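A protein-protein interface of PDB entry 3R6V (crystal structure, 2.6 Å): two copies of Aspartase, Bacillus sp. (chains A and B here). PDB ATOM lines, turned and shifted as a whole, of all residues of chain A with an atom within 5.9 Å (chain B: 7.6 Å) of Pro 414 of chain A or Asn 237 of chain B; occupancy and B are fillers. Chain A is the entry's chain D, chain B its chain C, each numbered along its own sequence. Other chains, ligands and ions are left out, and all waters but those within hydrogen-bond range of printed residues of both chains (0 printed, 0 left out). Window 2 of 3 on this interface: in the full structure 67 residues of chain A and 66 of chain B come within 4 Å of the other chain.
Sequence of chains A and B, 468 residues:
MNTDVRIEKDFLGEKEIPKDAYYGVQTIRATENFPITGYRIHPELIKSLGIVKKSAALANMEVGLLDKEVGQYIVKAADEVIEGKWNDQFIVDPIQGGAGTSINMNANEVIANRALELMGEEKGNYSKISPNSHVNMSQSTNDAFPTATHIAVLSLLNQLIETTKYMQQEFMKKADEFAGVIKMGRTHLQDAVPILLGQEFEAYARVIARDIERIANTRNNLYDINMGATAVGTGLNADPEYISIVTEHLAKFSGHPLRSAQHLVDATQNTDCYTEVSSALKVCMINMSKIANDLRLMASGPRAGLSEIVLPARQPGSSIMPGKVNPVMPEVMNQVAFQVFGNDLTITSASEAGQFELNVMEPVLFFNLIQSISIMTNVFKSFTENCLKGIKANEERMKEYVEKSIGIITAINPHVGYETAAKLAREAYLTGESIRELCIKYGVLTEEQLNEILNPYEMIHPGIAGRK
The backbone carbonyl oxygen of Thr 410 of chain A lies within hydrogen-bond range of the side-chain amide nitrogen of Asn 237 of chain B, 2.7 Å away.
The backbone carbonyl oxygen (O) of Ala 238 of chain B lies within hydrogen-bond range of the backbone NH (N) of Gly 463 of chain A, 3.1 Å away.
The backbone carbonyl oxygen (O) of Thr 234 of chain B lies close to the backbone nitrogen (N) of Pro 462 of chain A (3.5 Å).
OG1 of Thr 230 of chain B lies within hydrogen-bond range of N of Gly 235 of chain B (3.5 Å).
Among the printed residues, pairs that only touch across the chains: Pro 414 of chain A with Asn 237 of chain B (3.6 Å), His 461 of chain A with Thr 234 of chain B (3.4 Å), Pro 462 of chain A with Gly 235 of chain B (3.2 Å), Gly 463 of chain A with Gly 235 of chain B (3.8 Å) and Gly 463 of chain A with Asn 237 of chain B (3.8 Å).
Asn 237 of chain B touches three residues of chain A.
Printed residues of chain B within 4 Å of His 461 of chain A: Thr 234 (3.4 Å).
Of the printed residues of chain B, Pro 462 of chain A touches Thr 234 and Gly 235.
Of the printed residues of chain B, Gly 463 of chain A touches Gly 235 (3.8 Å), Asn 237 (3.8 Å) and Ala 238 (3.1 Å).
Of the printed residues of chain A, Ala 238 of chain B touches Gly 463.
Printed residues of chain A within 4 Å of Gly 235 of chain B: Pro 462 and Gly 463.
The nearest residue of chain A that does not touch Asn 237 of chain B is Ala 411 of chain A (4.2 Å).
Of the 12 printed residues of chain A, 5 touch a printed residue of chain B.
Printed residues of chain A that touch a printed residue of chain B: Thr 410, Pro 414, His 461, Pro 462 and Gly 463.
Of the 11 printed residues of chain B, 4 touch a printed residue of chain A.
Among the printed residues, no Asp or Glu carboxylate lies within 4 Å of a Lys or Arg side-chain nitrogen of the other chain.
No position is printed for both chains.
Of the 8 pairs that touch across the chains among the printed residues, none has its exchanged pair printed and touching as well.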
ATOM      1  N   ILE A 409      -5.612  26.421  -5.564  1.00  0.00           N
ATOM      2  CA  ILE A 409      -4.579  26.930  -6.467  1.00  0.00           C
ATOM      3  C   ILE A 409      -3.206  26.273  -6.229  1.00  0.00           C
ATOM      4  O   ILE A 409      -2.377  26.219  -7.135  1.00  0.00           O
ATOM      5  CB  ILE A 409      -4.494  28.498  -6.410  1.00  0.00           C
ATOM      6  CG1 ILE A 409      -3.821  29.077  -7.662  1.00  0.00           C
ATOM      7  CG2 ILE A 409      -3.823  28.976  -5.117  1.00  0.00           C
ATOM      8  CD1 ILE A 409      -4.668  29.016  -8.908  1.00  0.00           C
ATOM      9  N   THR A 410      -2.981  25.771  -5.016  1.00  0.00           N
ATOM     10  CA  THR A 410      -1.752  25.057  -4.694  1.00  0.00           C
ATOM     11  C   THR A 410      -1.603  23.807  -5.551  1.00  0.00           C
ATOM     12  O   THR A 410      -0.495  23.438  -5.919  1.00  0.00           O
ATOM     13  CB  THR A 410      -1.679  24.680  -3.205  1.00  0.00           C
ATOM     14  OG1 THR A 410      -1.976  25.831  -2.408  1.00  0.00           O
ATOM     15  CG2 THR A 410      -0.276  24.198  -2.839  1.00  0.00           C
ATOM     16  N   ALA A 411      -2.718  23.161  -5.876  1.00  0.00           N
ATOM     17  CA  ALA A 411      -2.677  21.967  -6.703  1.00  0.00           C
ATOM     18  C   ALA A 411      -2.421  22.324  -8.158  1.00  0.00           C
ATOM     19  O   ALA A 411      -1.922  21.507  -8.931  1.00  0.00           O
ATOM     20  CB  ALA A 411      -3.971  21.188  -6.569  1.00  0.00           C
ATOM     21  N   ILE A 412      -2.765  23.554  -8.519  1.00  0.00           N
ATOM     22  CA  ILE A 412      -2.668  24.043  -9.898  1.00  0.00           C
ATOM     23  C   ILE A 412      -1.321  24.718 -10.190  1.00  0.00           C
ATOM     24  O   ILE A 412      -0.793  24.594 -11.289  1.00  0.00           O
ATOM     25  CB  ILE A 412      -3.896  24.945 -10.226  1.00  0.00           C
ATOM     26  CG1 ILE A 412      -5.057  24.054 -10.679  1.00  0.00           C
ATOM     27  CG2 ILE A 412      -3.576  26.001 -11.269  1.00  0.00           C
ATOM     28  CD1 ILE A 412      -6.417  24.636 -10.457  1.00  0.00           C
ATOM     29  N   ASN A 413      -0.782  25.401  -9.182  1.00  0.00           N
ATOM     30  CA  ASN A 413       0.521  26.076  -9.192  1.00  0.00           C
ATOM     31  C   ASN A 413       1.607  25.512 -10.137  1.00  0.00           C
ATOM     32  O   ASN A 413       1.932  26.155 -11.132  1.00  0.00           O
ATOM     33  CB  ASN A 413       1.037  26.181  -7.745  1.00  0.00           C
ATOM     34  CG  ASN A 413       2.170  27.194  -7.568  1.00  0.00           C
ATOM     35  OD1 ASN A 413       2.592  27.876  -8.510  1.00  0.00           O
ATOM     36  ND2 ASN A 413       2.667  27.291  -6.337  1.00  0.00           N
ATOM     37  N   PRO A 414       2.149  24.307  -9.856  1.00  0.00           N
ATOM     38  CA  PRO A 414       3.310  23.896 -10.649  1.00  0.00           C
ATOM     39  C   PRO A 414       2.976  23.543 -12.105  1.00  0.00           C
ATOM     40  O   PRO A 414       3.887  23.305 -12.909  1.00  0.00           O
ATOM     41  CB  PRO A 414       3.817  22.666  -9.898  1.00  0.00           C
ATOM     42  CG  PRO A 414       2.578  22.050  -9.348  1.00  0.00           C
ATOM     43  CD  PRO A 414       1.672  23.207  -8.989  1.00  0.00           C
ATOM     44  N   HIS A 415       1.685  23.524 -12.438  1.00  0.00           N
ATOM     45  CA  HIS A 415       1.236  23.205 -13.795  1.00  0.00           C
ATOM     46  C   HIS A 415       1.127  24.433 -14.698  1.00  0.00           C
ATOM     47  O   HIS A 415       1.081  24.304 -15.918  1.00  0.00           O
ATOM     48  CB  HIS A 415      -0.109  22.480 -13.752  1.00  0.00           C
ATOM     49  CG  HIS A 415      -0.052  21.143 -13.083  1.00  0.00           C
ATOM     50  ND1 HIS A 415       0.533  20.042 -13.671  1.00  0.00           N
ATOM     51  CD2 HIS A 415      -0.515  20.727 -11.880  1.00  0.00           C
ATOM     52  CE1 HIS A 415       0.429  19.006 -12.857  1.00  0.00           C
ATOM     53  NE2 HIS A 415      -0.206  19.394 -11.767  1.00  0.00           N
ATOM     54  N   VAL A 416       1.083  25.616 -14.091  1.00  0.00           N
ATOM     55  CA  VAL A 416       0.873  26.875 -14.811  1.00  0.00           C
ATOM     56  C   VAL A 416       1.900  27.941 -14.432  1.00  0.00           C
ATOM     57  O   VAL A 416       1.702  29.126 -14.714  1.00  0.00           O
ATOM     58  CB  VAL A 416      -0.552  27.454 -14.555  1.00  0.00           C
ATOM     59  CG1 VAL A 416      -1.620  26.609 -15.236  1.00  0.00           C
ATOM     60  CG2 VAL A 416      -0.829  27.616 -13.049  1.00  0.00           C
ATOM     61  N   GLY A 417       2.982  27.523 -13.779  1.00  0.00           N
ATOM     62  CA  GLY A 417       3.999  28.445 -13.273  1.00  0.00           C
ATOM     63  C   GLY A 417       3.490  29.308 -12.133  1.00  0.00           C
ATOM     64  O   GLY A 417       2.290  29.584 -12.037  1.00  0.00           O
ATOM     65  N   HIS A 461      -2.382  13.347  -1.818  1.00  0.00           N
ATOM     66  CA  HIS A 461      -1.223  12.458  -1.737  1.00  0.00           C
ATOM     67  C   HIS A 461       0.008  12.999  -2.468  1.00  0.00           C
ATOM     68  O   HIS A 461      -0.126  13.810  -3.400  1.00  0.00           O
ATOM     69  CB  HIS A 461      -1.599  11.056  -2.197  1.00  0.00           C
ATOM     70  CG  HIS A 461      -2.430  10.324  -1.197  1.00  0.00           C
ATOM     71  ND1 HIS A 461      -3.793  10.161  -1.335  1.00  0.00           N
ATOM     72  CD2 HIS A 461      -2.098   9.757  -0.013  1.00  0.00           C
ATOM     73  CE1 HIS A 461      -4.259   9.500  -0.291  1.00  0.00           C
ATOM     74  NE2 HIS A 461      -3.251   9.240   0.524  1.00  0.00           N
ATOM     75  N   PRO A 462       1.210  12.573  -2.030  1.00  0.00           N
ATOM     76  CA  PRO A 462       2.472  13.074  -2.579  1.00  0.00           C
ATOM     77  C   PRO A 462       2.599  12.915  -4.101  1.00  0.00           C
ATOM     78  O   PRO A 462       2.099  11.943  -4.677  1.00  0.00           O
ATOM     79  CB  PRO A 462       3.525  12.239  -1.845  1.00  0.00           C
ATOM     80  CG  PRO A 462       2.889  11.899  -0.563  1.00  0.00           C
ATOM     81  CD  PRO A 462       1.444  11.659  -0.898  1.00  0.00           C
ATOM     82  N   GLY A 463       3.270  13.891  -4.720  1.00  0.00           N
ATOM     83  CA  GLY A 463       3.377  14.018  -6.177  1.00  0.00           C
ATOM     84  C   GLY A 463       3.150  15.459  -6.628  1.00  0.00           C
ATOM     85  O   GLY A 463       3.542  15.858  -7.734  1.00  0.00           O
ATOM     86  N   LEU B  65      15.978  21.032  -7.803  1.00  0.00           N
ATOM     87  CA  LEU B  65      14.995  22.096  -7.573  1.00  0.00           C
ATOM     88  C   LEU B  65      15.634  23.367  -7.016  1.00  0.00           C
ATOM     89  O   LEU B  65      15.127  24.471  -7.231  1.00  0.00           O
ATOM     90  CB  LEU B  65      13.846  21.601  -6.686  1.00  0.00           C
ATOM     91  CG  LEU B  65      12.668  21.014  -7.475  1.00  0.00           C
ATOM     92  CD1 LEU B  65      11.997  19.839  -6.755  1.00  0.00           C
ATOM     93  CD2 LEU B  65      11.661  22.114  -7.797  1.00  0.00           C
ATOM     94  N   SER B 138      10.595  23.753  -0.523  1.00  0.00           N
ATOM     95  CA  SER B 138      10.085  22.372  -0.373  1.00  0.00           C
ATOM     96  C   SER B 138       9.436  22.124   0.982  1.00  0.00           C
ATOM     97  O   SER B 138       8.851  21.053   1.238  1.00  0.00           O
ATOM     98  CB  SER B 138      11.184  21.325  -0.638  1.00  0.00           C
ATOM     99  OG  SER B 138      11.715  21.472  -1.944  1.00  0.00           O
ATOM    100  N   GLY B 228       8.386  16.911   4.661  1.00  0.00           N
ATOM    101  CA  GLY B 228       7.699  16.616   3.395  1.00  0.00           C
ATOM    102  C   GLY B 228       6.180  16.632   3.484  1.00  0.00           C
ATOM    103  O   GLY B 228       5.490  16.176   2.563  1.00  0.00           O
ATOM    104  N   THR B 230       4.232  19.319   3.737  1.00  0.00           N
ATOM    105  CA  THR B 230       3.673  20.598   3.268  1.00  0.00           C
ATOM    106  C   THR B 230       2.618  21.085   4.261  1.00  0.00           C
ATOM    107  O   THR B 230       2.621  20.650   5.402  1.00  0.00           O
ATOM    108  CB  THR B 230       3.183  20.566   1.785  1.00  0.00           C
ATOM    109  OG1 THR B 230       2.022  19.735   1.655  1.00  0.00           O
ATOM    110  CG2 THR B 230       4.280  20.043   0.868  1.00  0.00           C
ATOM    111  N   THR B 234      -0.593  16.391   3.635  1.00  0.00           N
ATOM    112  CA  THR B 234      -0.948  15.662   2.408  1.00  0.00           C
ATOM    113  C   THR B 234       0.210  15.508   1.429  1.00  0.00           C
ATOM    114  O   THR B 234       0.153  14.669   0.534  1.00  0.00           O
ATOM    115  CB  THR B 234      -2.103  16.324   1.653  1.00  0.00           C
ATOM    116  OG1 THR B 234      -1.804  17.708   1.438  1.00  0.00           O
ATOM    117  CG2 THR B 234      -3.395  16.192   2.429  1.00  0.00           C
ATOM    118  N   GLY B 235       1.249  16.324   1.601  1.00  0.00           N
ATOM    119  CA  GLY B 235       2.436  16.293   0.743  1.00  0.00           C
ATOM    120  C   GLY B 235       2.142  16.688  -0.690  1.00  0.00           C
ATOM    121  O   GLY B 235       2.663  16.086  -1.638  1.00  0.00           O
ATOM    122  N   LEU B 236       1.299  17.705  -0.839  1.00  0.00           N
ATOM    123  CA  LEU B 236       0.847  18.170  -2.138  1.00  0.00           C
ATOM    124  C   LEU B 236       1.980  18.866  -2.879  1.00  0.00           C
ATOM    125  O   LEU B 236       2.485  19.904  -2.437  1.00  0.00           O
ATOM    126  CB  LEU B 236      -0.359  19.093  -1.961  1.00  0.00           C
ATOM    127  CG  LEU B 236      -0.994  19.824  -3.142  1.00  0.00           C
ATOM    128  CD1 LEU B 236      -1.252  18.902  -4.336  1.00  0.00           C
ATOM    129  CD2 LEU B 236      -2.277  20.483  -2.676  1.00  0.00           C
ATOM    130  N   ASN B 237       2.376  18.270  -4.003  1.00  0.00           N
ATOM    131  CA  ASN B 237       3.517  18.736  -4.813  1.00  0.00           C
ATOM    132  C   ASN B 237       4.873  18.556  -4.138  1.00  0.00           C
ATOM    133  O   ASN B 237       5.856  19.169  -4.557  1.00  0.00           O
ATOM    134  CB  ASN B 237       3.352  20.191  -5.282  1.00  0.00           C
ATOM    135  CG  ASN B 237       2.044  20.434  -6.021  1.00  0.00           C
ATOM    136  OD1 ASN B 237       1.592  19.615  -6.837  1.00  0.00           O
ATOM    137  ND2 ASN B 237       1.428  21.576  -5.739  1.00  0.00           N
ATOM    138  N   ALA B 238       4.929  17.736  -3.090  1.00  0.00           N
ATOM    139  CA  ALA B 238       6.206  17.273  -2.573  1.00  0.00           C
ATOM    140  C   ALA B 238       6.719  16.131  -3.461  1.00  0.00           C
ATOM    141  O   ALA B 238       5.928  15.355  -4.007  1.00  0.00           O
ATOM    142  CB  ALA B 238       6.063  16.815  -1.142  1.00  0.00           C
ATOM    143  N   ASP B 239       8.041  16.052  -3.622  1.00  0.00           N
ATOM    144  CA  ASP B 239       8.690  14.958  -4.353  1.00  0.00           C
ATOM    145  C   ASP B 239       9.087  13.862  -3.360  1.00  0.00           C
ATOM    146  O   ASP B 239       9.879  14.124  -2.460  1.00  0.00           O
ATOM    147  CB  ASP B 239       9.933  15.490  -5.072  1.00  0.00           C
ATOM    148  CG  ASP B 239      10.615  14.440  -5.949  1.00  0.00           C
ATOM    149  OD1 ASP B 239      11.559  14.809  -6.687  1.00  0.00           O
ATOM    150  OD2 ASP B 239      10.217  13.252  -5.915  1.00  0.00           O
ATOM    151  N   PRO B 240       8.538  12.633  -3.512  1.00  0.00           N
ATOM    152  CA  PRO B 240       8.879  11.537  -2.581  1.00  0.00           C
ATOM    153  C   PRO B 240      10.381  11.334  -2.396  1.00  0.00           C
ATOM    154  O   PRO B 240      10.814  10.825  -1.357  1.00  0.00           O
ATOM    155  CB  PRO B 240       8.261  10.304  -3.245  1.00  0.00           C
ATOM    156  CG  PRO B 240       7.092  10.848  -4.011  1.00  0.00           C
ATOM    157  CD  PRO B 240       7.523  12.214  -4.501  1.00  0.00           C
